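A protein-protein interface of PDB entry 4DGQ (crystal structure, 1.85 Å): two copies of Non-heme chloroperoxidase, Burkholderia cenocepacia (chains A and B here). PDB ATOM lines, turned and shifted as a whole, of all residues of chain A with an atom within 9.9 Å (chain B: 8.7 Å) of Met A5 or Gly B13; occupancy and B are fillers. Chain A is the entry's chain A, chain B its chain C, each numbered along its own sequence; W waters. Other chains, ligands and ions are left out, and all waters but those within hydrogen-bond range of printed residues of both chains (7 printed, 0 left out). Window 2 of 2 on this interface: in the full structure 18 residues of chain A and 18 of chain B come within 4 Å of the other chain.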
ATOM      1  N   SER A   4     -25.625 -25.180  -3.333  1.00  0.00           N
ATOM      2  CA  SER A   4     -24.466 -25.412  -2.452  1.00  0.00           C
ATOM      3  C   SER A   4     -24.583 -24.554  -1.131  1.00  0.00           C
ATOM      4  O   SER A   4     -25.167 -23.426  -1.097  1.00  0.00           O
ATOM      5  CB  SER A   4     -23.169 -25.164  -3.249  1.00  0.00           C
ATOM      6  OG  SER A   4     -22.042 -25.130  -2.397  1.00  0.00           O
ATOM      7  N   MET A   5     -24.132 -25.139  -0.022  1.00  0.00           N
ATOM      8  CA  MET A   5     -24.358 -24.543   1.277  1.00  0.00           C
ATOM      9  C   MET A   5     -23.477 -23.312   1.369  1.00  0.00           C
ATOM     10  O   MET A   5     -22.301 -23.388   1.135  1.00  0.00           O
ATOM     11  CB  MET A   5     -23.977 -25.552   2.385  1.00  0.00           C
ATOM     12  CG  MET A   5     -24.097 -25.035   3.794  1.00  0.00           C
ATOM     13  SD  MET A   5     -23.897 -26.377   5.001  1.00  0.00           S
ATOM     14  CE  MET A   5     -25.389 -27.367   4.867  1.00  0.00           C
ATOM     15  N   GLY A   6     -24.038 -22.188   1.741  1.00  0.00           N
ATOM     16  CA  GLY A   6     -23.201 -21.006   2.016  1.00  0.00           C
ATOM     17  C   GLY A   6     -22.691 -20.217   0.823  1.00  0.00           C
ATOM     18  O   GLY A   6     -21.876 -19.322   1.000  1.00  0.00           O
ATOM     19  N   THR A   7     -23.207 -20.480  -0.375  1.00  0.00           N
ATOM     20  CA  THR A   7     -22.971 -19.599  -1.517  1.00  0.00           C
ATOM     21  C   THR A   7     -24.247 -19.380  -2.336  1.00  0.00           C
ATOM     22  O   THR A   7     -25.106 -20.274  -2.394  1.00  0.00           O
ATOM     23  CB  THR A   7     -21.859 -20.122  -2.446  1.00  0.00           C
ATOM     24  OG1 THR A   7     -22.268 -21.364  -3.048  1.00  0.00           O
ATOM     25  CG2 THR A   7     -20.524 -20.340  -1.653  1.00  0.00           C
ATOM     26  N   VAL A   8     -24.364 -18.191  -2.927  1.00  0.00           N
ATOM     27  CA  VAL A   8     -25.385 -17.856  -3.912  1.00  0.00           C
ATOM     28  C   VAL A   8     -24.723 -17.040  -5.023  1.00  0.00           C
ATOM     29  O   VAL A   8     -23.866 -16.186  -4.770  1.00  0.00           O
ATOM     30  CB  VAL A   8     -26.526 -17.057  -3.269  1.00  0.00           C
ATOM     31  CG1 VAL A   8     -26.035 -15.769  -2.669  1.00  0.00           C
ATOM     32  CG2 VAL A   8     -27.708 -16.834  -4.268  1.00  0.00           C
ATOM     33  N   THR A   9     -25.099 -17.300  -6.253  1.00  0.00           N
ATOM     34  CA  THR A   9     -24.606 -16.546  -7.373  1.00  0.00           C
ATOM     35  C   THR A   9     -25.636 -15.484  -7.717  1.00  0.00           C
ATOM     36  O   THR A   9     -26.814 -15.802  -7.900  1.00  0.00           O
ATOM     37  CB  THR A   9     -24.358 -17.485  -8.544  1.00  0.00           C
ATOM     38  OG1 THR A   9     -23.382 -18.459  -8.138  1.00  0.00           O
ATOM     39  CG2 THR A   9     -23.864 -16.699  -9.802  1.00  0.00           C
ATOM     40  N   GLU A  15     -20.350 -14.669  -7.034  1.00  0.00           N
ATOM     41  CA  GLU A  15     -20.614 -15.619  -5.988  1.00  0.00           C
ATOM     42  C   GLU A  15     -20.461 -14.920  -4.631  1.00  0.00           C
ATOM     43  O   GLU A  15     -19.387 -14.365  -4.311  1.00  0.00           O
ATOM     44  CB  GLU A  15     -19.657 -16.813  -6.079  1.00  0.00           C
ATOM     45  CG  GLU A  15     -19.906 -17.793  -4.956  1.00  0.00           C
ATOM     46  CD  GLU A  15     -19.110 -19.089  -5.111  1.00  0.00           C
ATOM     47  OE1 GLU A  15     -18.062 -19.271  -4.438  1.00  0.00           O
ATOM     48  OE2 GLU A  15     -19.543 -19.909  -5.930  1.00  0.00           O
ATOM     49  N   ILE A  16     -21.549 -14.925  -3.870  1.00  0.00           N
ATOM     50  CA  ILE A  16     -21.588 -14.345  -2.527  1.00  0.00           C
ATOM     51  C   ILE A  16     -21.597 -15.466  -1.480  1.00  0.00           C
ATOM     52  O   ILE A  16     -22.487 -16.355  -1.508  1.00  0.00           O
ATOM     53  CB  ILE A  16     -22.826 -13.450  -2.315  1.00  0.00           C
ATOM     54  CG1 ILE A  16     -22.794 -12.273  -3.316  1.00  0.00           C
ATOM     55  CG2 ILE A  16     -22.925 -12.997  -0.838  1.00  0.00           C
ATOM     56  CD1 ILE A  16     -21.713 -11.215  -3.095  1.00  0.00           C
ATOM     57  N   PHE A  17     -20.599 -15.444  -0.611  1.00  0.00           N
ATOM     58  CA  PHE A  17     -20.445 -16.351   0.519  1.00  0.00           C
ATOM     59  C   PHE A  17     -21.336 -15.861   1.673  1.00  0.00           C
ATOM     60  O   PHE A  17     -21.419 -14.649   1.943  1.00  0.00           O
ATOM     61  CB  PHE A  17     -18.992 -16.420   1.003  1.00  0.00           C
ATOM     62  CG  PHE A  17     -18.824 -17.219   2.250  1.00  0.00           C
ATOM     63  CD1 PHE A  17     -18.642 -18.587   2.166  1.00  0.00           C
ATOM     64  CD2 PHE A  17     -18.963 -16.630   3.484  1.00  0.00           C
ATOM     65  CE1 PHE A  17     -18.526 -19.360   3.317  1.00  0.00           C
ATOM     66  CE2 PHE A  17     -18.847 -17.377   4.646  1.00  0.00           C
ATOM     67  CZ  PHE A  17     -18.636 -18.750   4.557  1.00  0.00           C
ATOM     68  N   TYR A  18     -21.965 -16.799   2.361  1.00  0.00           N
ATOM     69  CA  TYR A  18     -22.723 -16.453   3.558  1.00  0.00           C
ATOM     70  C   TYR A  18     -22.714 -17.599   4.552  1.00  0.00           C
ATOM     71  O   TYR A  18     -22.513 -18.771   4.201  1.00  0.00           O
ATOM     72  CB  TYR A  18     -24.158 -16.023   3.215  1.00  0.00           C
ATOM     73  CG  TYR A  18     -24.952 -17.105   2.570  1.00  0.00           C
ATOM     74  CD1 TYR A  18     -25.010 -17.223   1.216  1.00  0.00           C
ATOM     75  CD2 TYR A  18     -25.642 -18.026   3.342  1.00  0.00           C
ATOM     76  CE1 TYR A  18     -25.702 -18.243   0.608  1.00  0.00           C
ATOM     77  CE2 TYR A  18     -26.346 -19.049   2.774  1.00  0.00           C
ATOM     78  CZ  TYR A  18     -26.381 -19.149   1.388  1.00  0.00           C
ATOM     79  OH  TYR A  18     -27.064 -20.151   0.806  1.00  0.00           O
ATOM     80  N   LYS A  19     -22.900 -17.230   5.808  1.00  0.00           N
ATOM     81  CA  LYS A  19     -23.186 -18.132   6.891  1.00  0.00           C
ATOM     82  C   LYS A  19     -24.694 -18.062   7.178  1.00  0.00           C
ATOM     83  O   LYS A  19     -25.275 -16.971   7.168  1.00  0.00           O
ATOM     84  CB  LYS A  19     -22.394 -17.648   8.136  1.00  0.00           C
ATOM     85  CG  LYS A  19     -20.886 -17.545   7.921  1.00  0.00           C
ATOM     86  CD  LYS A  19     -20.138 -17.036   9.159  1.00  0.00           C
ATOM     87  CE  LYS A  19     -18.629 -16.827   8.921  1.00  0.00           C
ATOM     88  NZ  LYS A  19     -17.760 -17.249  10.065  1.00  0.00           N
ATOM     89  N   ASP A  20     -25.339 -19.205   7.387  1.00  0.00           N
ATOM     90  CA  ASP A  20     -26.728 -19.283   7.784  1.00  0.00           C
ATOM     91  C   ASP A  20     -26.828 -20.342   8.870  1.00  0.00           C
ATOM     92  O   ASP A  20     -26.758 -21.541   8.618  1.00  0.00           O
ATOM     93  CB  ASP A  20     -27.591 -19.613   6.564  1.00  0.00           C
ATOM     94  CG  ASP A  20     -29.019 -19.893   6.900  1.00  0.00           C
ATOM     95  OD1 ASP A  20     -29.491 -19.616   8.022  1.00  0.00           O
ATOM     96  OD2 ASP A  20     -29.697 -20.423   5.996  1.00  0.00           O
ATOM     97  N   TRP A  21     -26.958 -19.890  10.104  1.00  0.00           N
ATOM     98  CA  TRP A  21     -26.906 -20.770  11.266  1.00  0.00           C
ATOM     99  C   TRP A  21     -28.187 -20.667  12.067  1.00  0.00           C
ATOM    100  O   TRP A  21     -28.691 -19.548  12.331  1.00  0.00           O
ATOM    101  CB  TRP A  21     -25.756 -20.370  12.169  1.00  0.00           C
ATOM    102  CG  TRP A  21     -24.378 -20.436  11.574  1.00  0.00           C
ATOM    103  CD1 TRP A  21     -23.970 -21.073  10.404  1.00  0.00           C
ATOM    104  CD2 TRP A  21     -23.183 -19.916  12.167  1.00  0.00           C
ATOM    105  NE1 TRP A  21     -22.618 -20.941  10.236  1.00  0.00           N
ATOM    106  CE2 TRP A  21     -22.091 -20.265  11.283  1.00  0.00           C
ATOM    107  CE3 TRP A  21     -22.903 -19.189  13.340  1.00  0.00           C
ATOM    108  CZ2 TRP A  21     -20.775 -19.887  11.555  1.00  0.00           C
ATOM    109  CZ3 TRP A  21     -21.585 -18.821  13.595  1.00  0.00           C
ATOM    110  CH2 TRP A  21     -20.543 -19.181  12.726  1.00  0.00           C
ATOM    111  N   ARG A  24     -34.445 -23.467  11.353  1.00  0.00           N
ATOM    112  CA  ARG A  24     -34.976 -22.886  10.134  1.00  0.00           C
ATOM    113  C   ARG A  24     -36.228 -22.031  10.347  1.00  0.00           C
ATOM    114  O   ARG A  24     -36.491 -21.122   9.598  1.00  0.00           O
ATOM    115  CB  ARG A  24     -35.264 -23.957   9.074  1.00  0.00           C
ATOM    116  CG  ARG A  24     -34.279 -23.909   7.912  1.00  0.00           C
ATOM    117  CD  ARG A  24     -32.944 -24.562   8.257  1.00  0.00           C
ATOM    118  NE  ARG A  24     -32.020 -23.720   9.003  1.00  0.00           N
ATOM    119  CZ  ARG A  24     -31.187 -22.830   8.458  1.00  0.00           C
ATOM    120  NH1 ARG A  24     -31.186 -22.629   7.137  1.00  0.00           N
ATOM    121  NH2 ARG A  24     -30.357 -22.145   9.230  1.00  0.00           N
ATOM    122  N   ARG A  66     -14.686 -14.301   1.223  1.00  0.00           N
ATOM    123  CA  ARG A  66     -14.782 -15.481   0.350  1.00  0.00           C
ATOM    124  C   ARG A  66     -15.684 -15.234  -0.868  1.00  0.00           C
ATOM    125  O   ARG A  66     -15.907 -16.166  -1.665  1.00  0.00           O
ATOM    126  CB  ARG A  66     -15.329 -16.671   1.166  1.00  0.00           C
ATOM    127  CG  ARG A  66     -14.331 -17.103   2.248  1.00  0.00           C
ATOM    128  CD  ARG A  66     -15.016 -17.593   3.512  1.00  0.00           C
ATOM    129  NE  ARG A  66     -15.634 -16.439   4.213  1.00  0.00           N
ATOM    130  CZ  ARG A  66     -15.798 -16.293   5.518  1.00  0.00           C
ATOM    131  NH1 ARG A  66     -15.341 -17.197   6.395  1.00  0.00           N
ATOM    132  NH2 ARG A  66     -16.399 -15.200   5.974  1.00  0.00           N
ATOM    133  N   LYS A  89     -32.624 -16.082  -1.917  1.00  0.00           N
ATOM    134  CA  LYS A  89     -32.324 -17.521  -1.855  1.00  0.00           C
ATOM    135  C   LYS A  89     -32.863 -18.130  -0.546  1.00  0.00           C
ATOM    136  O   LYS A  89     -33.476 -19.187  -0.531  1.00  0.00           O
ATOM    137  CB  LYS A  89     -30.812 -17.793  -1.962  1.00  0.00           C
ATOM    138  CG  LYS A  89     -30.550 -19.301  -1.847  1.00  0.00           C
ATOM    139  CD  LYS A  89     -29.122 -19.697  -2.019  1.00  0.00           C
ATOM    140  CE  LYS A  89     -28.920 -21.211  -1.857  1.00  0.00           C
ATOM    141  NZ  LYS A  89     -27.460 -21.452  -1.756  1.00  0.00           N
ATOM    142  N   LEU A  90     -32.677 -17.447   0.567  1.00  0.00           N
ATOM    143  CA  LEU A  90     -33.020 -18.054   1.826  1.00  0.00           C
ATOM    144  C   LEU A  90     -34.486 -17.870   2.275  1.00  0.00           C
ATOM    145  O   LEU A  90     -34.982 -18.549   3.206  1.00  0.00           O
ATOM    146  CB  LEU A  90     -32.053 -17.558   2.891  1.00  0.00           C
ATOM    147  CG  LEU A  90     -30.552 -17.800   2.717  1.00  0.00           C
ATOM    148  CD1 LEU A  90     -29.807 -17.247   3.946  1.00  0.00           C
ATOM    149  CD2 LEU A  90     -30.252 -19.301   2.471  1.00  0.00           C
ATOM    150  N   VAL B   8     -16.370 -33.335  -1.498  1.00  0.00           N
ATOM    151  CA  VAL B   8     -17.507 -34.272  -1.569  1.00  0.00           C
ATOM    152  C   VAL B   8     -18.660 -33.671  -0.777  1.00  0.00           C
ATOM    153  O   VAL B   8     -18.427 -33.058   0.261  1.00  0.00           O
ATOM    154  CB  VAL B   8     -17.153 -35.688  -1.062  1.00  0.00           C
ATOM    155  CG1 VAL B   8     -16.616 -35.698   0.370  1.00  0.00           C
ATOM    156  CG2 VAL B   8     -18.366 -36.655  -1.261  1.00  0.00           C
ATOM    157  N   THR B   9     -19.891 -33.849  -1.253  1.00  0.00           N
ATOM    158  CA  THR B   9     -21.055 -33.353  -0.539  1.00  0.00           C
ATOM    159  C   THR B   9     -21.711 -34.528   0.172  1.00  0.00           C
ATOM    160  O   THR B   9     -22.007 -35.551  -0.440  1.00  0.00           O
ATOM    161  CB  THR B   9     -22.042 -32.708  -1.526  1.00  0.00           C
ATOM    162  OG1 THR B   9     -21.407 -31.565  -2.086  1.00  0.00           O
ATOM    163  CG2 THR B   9     -23.376 -32.252  -0.809  1.00  0.00           C
ATOM    164  N   THR B  10     -21.932 -34.397   1.452  1.00  0.00           N
ATOM    165  CA  THR B  10     -22.504 -35.452   2.235  1.00  0.00           C
ATOM    166  C   THR B  10     -24.026 -35.536   1.965  1.00  0.00           C
ATOM    167  O   THR B  10     -24.608 -34.631   1.339  1.00  0.00           O
ATOM    168  CB  THR B  10     -22.329 -35.184   3.735  1.00  0.00           C
ATOM    169  OG1 THR B  10     -23.147 -34.047   4.083  1.00  0.00           O
ATOM    170  CG2 THR B  10     -20.876 -34.970   4.130  1.00  0.00           C
ATOM    171  N   LYS B  11     -24.646 -36.619   2.450  1.00  0.00           N
ATOM    172  CA  LYS B  11     -26.111 -36.833   2.412  1.00  0.00           C
ATOM    173  C   LYS B  11     -26.872 -35.652   2.968  1.00  0.00           C
ATOM    174  O   LYS B  11     -27.954 -35.336   2.462  1.00  0.00           O
ATOM    175  CB  LYS B  11     -26.522 -38.090   3.222  1.00  0.00           C
ATOM    176  N   ASP B  12     -26.324 -35.003   4.003  1.00  0.00           N
ATOM    177  CA  ASP B  12     -26.968 -33.836   4.606  1.00  0.00           C
ATOM    178  C   ASP B  12     -26.518 -32.452   4.039  1.00  0.00           C
ATOM    179  O   ASP B  12     -26.765 -31.415   4.676  1.00  0.00           O
ATOM    180  CB  ASP B  12     -26.960 -33.913   6.166  1.00  0.00           C
ATOM    181  CG  ASP B  12     -25.538 -34.088   6.815  1.00  0.00           C
ATOM    182  OD1 ASP B  12     -24.576 -34.627   6.202  1.00  0.00           O
ATOM    183  OD2 ASP B  12     -25.382 -33.690   8.001  1.00  0.00           O
ATOM    184  N   GLY B  13     -25.938 -32.428   2.828  1.00  0.00           N
ATOM    185  CA  GLY B  13     -25.609 -31.174   2.119  1.00  0.00           C
ATOM    186  C   GLY B  13     -24.367 -30.418   2.603  1.00  0.00           C
ATOM    187  O   GLY B  13     -24.155 -29.261   2.243  1.00  0.00           O
ATOM    188  N   VAL B  14     -23.515 -31.066   3.401  1.00  0.00           N
ATOM    189  CA  VAL B  14     -22.258 -30.484   3.867  1.00  0.00           C
ATOM    190  C   VAL B  14     -21.128 -30.804   2.856  1.00  0.00           C
ATOM    191  O   VAL B  14     -20.964 -31.950   2.431  1.00  0.00           O
ATOM    192  CB  VAL B  14     -21.863 -31.034   5.251  1.00  0.00           C
ATOM    193  CG1 VAL B  14     -20.494 -30.460   5.723  1.00  0.00           C
ATOM    194  CG2 VAL B  14     -22.968 -30.726   6.271  1.00  0.00           C
ATOM    195  N   GLU B  15     -20.376 -29.770   2.464  1.00  0.00           N
ATOM    196  CA  GLU B  15     -19.267 -29.950   1.607  1.00  0.00           C
ATOM    197  C   GLU B  15     -18.045 -30.213   2.487  1.00  0.00           C
ATOM    198  O   GLU B  15     -17.714 -29.384   3.349  1.00  0.00           O
ATOM    199  CB  GLU B  15     -19.070 -28.724   0.731  1.00  0.00           C
ATOM    200  CG  GLU B  15     -17.911 -28.892  -0.250  1.00  0.00           C
ATOM    201  CD  GLU B  15     -17.798 -27.715  -1.216  1.00  0.00           C
ATOM    202  OE1 GLU B  15     -18.528 -27.712  -2.222  1.00  0.00           O
ATOM    203  OE2 GLU B  15     -16.983 -26.780  -0.971  1.00  0.00           O
ATOM    204  N   ILE B  16     -17.387 -31.338   2.252  1.00  0.00           N
ATOM    205  CA  ILE B  16     -16.186 -31.735   2.989  1.00  0.00           C
ATOM    206  C   ILE B  16     -15.013 -31.607   2.042  1.00  0.00           C
ATOM    207  O   ILE B  16     -15.004 -32.211   0.989  1.00  0.00           O
ATOM    208  CB  ILE B  16     -16.288 -33.193   3.475  1.00  0.00           C
ATOM    209  CG1 ILE B  16     -17.450 -33.321   4.504  1.00  0.00           C
ATOM    210  CG2 ILE B  16     -14.941 -33.710   4.073  1.00  0.00           C
ATOM    211  CD1 ILE B  16     -17.171 -32.548   5.801  1.00  0.00           C
ATOM    212  N   ARG B  62     -16.280 -31.154   9.353  1.00  0.00           N
ATOM    213  CA  ARG B  62     -17.339 -30.177   9.101  1.00  0.00           C
ATOM    214  C   ARG B  62     -17.103 -28.913   9.940  1.00  0.00           C
ATOM    215  O   ARG B  62     -16.759 -28.986  11.115  1.00  0.00           O
ATOM    216  CB  ARG B  62     -18.727 -30.778   9.373  1.00  0.00           C
ATOM    217  CG  ARG B  62     -18.961 -31.247  10.818  1.00  0.00           C
ATOM    218  CD  ARG B  62     -20.490 -31.418  11.078  1.00  0.00           C
ATOM    219  NE  ARG B  62     -21.048 -32.387  10.132  1.00  0.00           N
ATOM    220  CZ  ARG B  62     -22.316 -32.472   9.753  1.00  0.00           C
ATOM    221  NH1 ARG B  62     -23.258 -31.644  10.214  1.00  0.00           N
ATOM    222  NH2 ARG B  62     -22.628 -33.418   8.844  1.00  0.00           N
ATOM    223  N   GLY B  63     -17.256 -27.761   9.328  1.00  0.00           N
ATOM    224  CA  GLY B  63     -17.054 -26.514  10.052  1.00  0.00           C
ATOM    225  C   GLY B  63     -15.635 -26.167  10.370  1.00  0.00           C
ATOM    226  O   GLY B  63     -15.402 -25.223  11.103  1.00  0.00           O
ATOM    227  N   ARG B  66     -11.611 -25.816   5.224  1.00  0.00           N
ATOM    228  CA  ARG B  66     -12.324 -25.426   4.000  1.00  0.00           C
ATOM    229  C   ARG B  66     -13.664 -26.163   3.840  1.00  0.00           C
ATOM    230  O   ARG B  66     -14.299 -26.074   2.818  1.00  0.00           O
ATOM    231  CB  ARG B  66     -11.426 -25.704   2.795  1.00  0.00           C
ATOM    232  CG  ARG B  66     -10.166 -24.824   2.782  1.00  0.00           C
ATOM    233  CD  ARG B  66      -8.890 -25.600   2.326  1.00  0.00           C
ATOM    234  NE  ARG B  66      -8.465 -26.581   3.323  1.00  0.00           N
ATOM    235  CZ  ARG B  66      -7.233 -26.997   3.555  1.00  0.00           C
ATOM    236  NH1 ARG B  66      -6.184 -26.428   2.924  1.00  0.00           N
ATOM    237  NH2 ARG B  66      -7.053 -27.949   4.459  1.00  0.00           N
ATOM    238  N   SER B  67     -14.070 -26.920   4.841  1.00  0.00           N
ATOM    239  CA  SER B  67     -15.380 -27.578   4.795  1.00  0.00           C
ATOM    240  C   SER B  67     -16.499 -26.591   5.204  1.00  0.00           C
ATOM    241  O   SER B  67     -16.256 -25.528   5.816  1.00  0.00           O
ATOM    242  CB  SER B  67     -15.364 -28.819   5.687  1.00  0.00           C
ATOM    243  OG  SER B  67     -14.504 -29.864   5.183  1.00  0.00           O
ATOM    244  N   SER B  68     -17.722 -26.894   4.778  1.00  0.00           N
ATOM    245  CA  SER B  68     -18.871 -26.011   4.999  1.00  0.00           C
ATOM    246  C   SER B  68     -19.047 -25.633   6.480  1.00  0.00           C
ATOM    247  O   SER B  68     -18.913 -26.462   7.370  1.00  0.00           O
ATOM    248  CB  SER B  68     -20.205 -26.670   4.560  1.00  0.00           C
ATOM    249  OG  SER B  68     -20.121 -27.028   3.219  1.00  0.00           O
ATOM    250  N   GLN B  69     -19.391 -24.380   6.714  1.00  0.00           N
ATOM    251  CA  GLN B  69     -19.678 -23.887   8.060  1.00  0.00           C
ATOM    252  C   GLN B  69     -21.151 -24.201   8.415  1.00  0.00           C
ATOM    253  O   GLN B  69     -21.967 -23.339   8.625  1.00  0.00           O
ATOM    254  CB  GLN B  69     -19.350 -22.409   8.157  1.00  0.00           C
ATOM    255  CG  GLN B  69     -17.867 -22.112   7.846  1.00  0.00           C
ATOM    256  CD  GLN B  69     -17.338 -20.850   8.497  1.00  0.00           C
ATOM    257  OE1 GLN B  69     -18.056 -20.136   9.236  1.00  0.00           O
ATOM    258  NE2 GLN B  69     -16.041 -20.614   8.319  1.00  0.00           N
ATOM    259  N   VAL B  70     -21.445 -25.484   8.473  1.00  0.00           N
ATOM    260  CA  VAL B  70     -22.764 -25.987   8.854  1.00  0.00           C
ATOM    261  C   VAL B  70     -22.930 -25.728  10.362  1.00  0.00           C
ATOM    262  O   VAL B  70     -21.960 -25.836  11.156  1.00  0.00           O
ATOM    263  CB  VAL B  70     -22.892 -27.510   8.498  1.00  0.00           C
ATOM    264  CG1 VAL B  70     -21.807 -28.391   9.187  1.00  0.00           C
ATOM    265  CG2 VAL B  70     -24.318 -28.014   8.766  1.00  0.00           C
ATOM    266  N   TRP B  71     -24.126 -25.370  10.776  1.00  0.00           N
ATOM    267  CA  TRP B  71     -24.318 -24.962  12.164  1.00  0.00           C
ATOM    268  C   TRP B  71     -24.536 -26.094  13.141  1.00  0.00           C
ATOM    269  O   TRP B  71     -24.313 -25.927  14.346  1.00  0.00           O
ATOM    270  CB  TRP B  71     -25.423 -23.934  12.260  1.00  0.00           C
ATOM    271  CG  TRP B  71     -26.804 -24.508  12.237  1.00  0.00           C
ATOM    272  CD1 TRP B  71     -27.574 -24.891  11.130  1.00  0.00           C
ATOM    273  CD2 TRP B  71     -27.645 -24.763  13.416  1.00  0.00           C
ATOM    274  NE1 TRP B  71     -28.821 -25.346  11.553  1.00  0.00           N
ATOM    275  CE2 TRP B  71     -28.905 -25.312  12.920  1.00  0.00           C
ATOM    276  CE3 TRP B  71     -27.467 -24.614  14.775  1.00  0.00           C
ATOM    277  CZ2 TRP B  71     -29.945 -25.666  13.781  1.00  0.00           C
ATOM    278  CZ3 TRP B  71     -28.504 -25.001  15.630  1.00  0.00           C
ATOM    279  CH2 TRP B  71     -29.721 -25.486  15.127  1.00  0.00           C
ATOM    280  N   ASP B  72     -24.953 -27.259  12.647  1.00  0.00           N
ATOM    281  CA  ASP B  72     -25.320 -28.349  13.530  1.00  0.00           C
ATOM    282  C   ASP B  72     -24.623 -29.664  13.145  1.00  0.00           C
ATOM    283  O   ASP B  72     -23.786 -29.697  12.226  1.00  0.00           O
ATOM    284  CB  ASP B  72     -26.861 -28.511  13.589  1.00  0.00           C
ATOM    285  CG  ASP B  72     -27.465 -28.751  12.259  1.00  0.00           C
ATOM    286  OD1 ASP B  72     -26.728 -28.705  11.262  1.00  0.00           O
ATOM    287  OD2 ASP B  72     -28.694 -28.972  12.196  1.00  0.00           O
ATOM    288  N   ASP B  82     -19.327 -38.159   7.896  1.00  0.00           N
ATOM    289  CA  ASP B  82     -18.661 -37.296   6.937  1.00  0.00           C
ATOM    290  C   ASP B  82     -17.343 -37.981   6.429  1.00  0.00           C
ATOM    291  O   ASP B  82     -17.030 -37.910   5.252  1.00  0.00           O
ATOM    292  CB  ASP B  82     -18.309 -35.927   7.564  1.00  0.00           C
ATOM    293  CG  ASP B  82     -19.549 -35.099   8.036  1.00  0.00           C
ATOM    294  OD1 ASP B  82     -20.748 -35.359   7.678  1.00  0.00           O
ATOM    295  OD2 ASP B  82     -19.303 -34.112   8.789  1.00  0.00           O
HETATM  296  O   HOH W   1     -25.641 -24.273   8.514  1.00  0.00           O
HETATM  297  O   HOH W   2     -23.017 -27.919   0.026  1.00  0.00           O
HETATM  298  O   HOH W   3     -23.764 -21.737   6.897  1.00  0.00           O
HETATM  299  O   HOH W   4     -20.251 -24.968   1.881  1.00  0.00           O
HETATM  300  O   HOH W   5     -14.595 -18.344   9.855  1.00  0.00           O
HETATM  301  O   HOH W   6     -21.106 -23.269  11.764  1.00  0.00           O
HETATM  302  O   HOH W   7     -31.144 -26.357  10.205  1.00  0.00           O
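The indole nitrogen (NE1) of Trp A21 sits at hydrogen-bond distance from the backbone carbonyl oxygen (O) of Gln B69 (3.0 Å). The side-chain amino group (NZ) of Lys A19 is in hydrogen-bond range of the side-chain amide oxygen (OE1) of Gln B69, at 3.0 Å.
OG1 of Thr B10 is in hydrogen-bond range of N of Gly B13. The backbone NH (N) of Gly B63 lies within hydrogen-bond range of the backbone carbonyl oxygen (O) of Ser B68 (2.9 Å). The side-chain hydroxyl (OG) of Ser B68 sits at hydrogen-bond distance from the backbone NH (N) of Glu B15, 2.9 Å away.
Among the printed residues, pairs that only touch across the chains: Met A5 with Gly B13, Met A5 with Ser B68, Met A5 with Val B70, Trp A21 with Trp B71 and Arg A66 with Gln B69.
Met A5 touches just these residues of chain B: Gly B13, Ser B68 and Val B70. Gly A6 touches none of the printed residues of chain B. No residue of chain A comes within 4 Å of Thr B10. No residue of chain A comes within 4 Å of Lys B11. No residue of chain A comes within 4 Å of Asp B12. Of the printed residues of chain B, Trp A21 touches Gln B69 (3.0 Å) and Trp B71 (3.6 Å). Printed residues of chain A within 4 Å of Trp B71: Trp A21. Of the printed residues of chain B, Arg A66 touches Gln B69 (3.98 Å). Printed residues of chain A within 4 Å of Gln B69: Lys A19, Trp A21 and Arg A66. Of the printed residues of chain A, Val B70 touches Met A5. Asp A20 touches none of the printed residues of chain B. Val A8 touches none of the printed residues of chain B. The nearest residue of chain A that does not touch Gly B13 is Ser A4 (5.8 Å).
Of the 17 printed residues of chain A, 4 touch a printed residue of chain B. Hydrophobic or aromatic side chains of chain A that line the printed part of chain B: Met A5 and Trp A21. Of the 19 printed residues of chain B, 5 touch a printed residue of chain A. Among the printed residues, no Asp or Glu carboxylate lies within 4 Å of a Lys or Arg side-chain nitrogen of the other chain.
Positions printed for both chains: 8, 9, 15, 16 and 66. Of the 7 pairs that touch across the chains among the printed residues, none has its exchanged pair printed and touching as well.
Water W4 bridges OG of Ser B68 (2.5 Å) and O of Met A5 (2.7 Å). Water W2 lies within hydrogen-bond range of the backbone carbonyl oxygen of Gly B13 (2.8 Å) and the backbone NH of Met A5 (3.0 Å). Water W7 lies within hydrogen-bond range of NE1 of Trp B71 (2.9 Å) and NE of Arg A24 (3.0 Å). Water W1 lies within hydrogen-bond range of the backbone NH (N) of Trp B71 (2.9 Å) and the backbone carbonyl oxygen (O) of Asp A20 (3.0 Å). Water W3 lies within hydrogen-bond range of the backbone carbonyl oxygen of Gln B69 (3.0 Å) and the backbone NH of Asp A20 (3.0 Å). Water W5 bridges the side-chain amide nitrogen of Gln B69 (3.1 Å) and the side-chain amino group of Lys A19 (3.4 Å).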
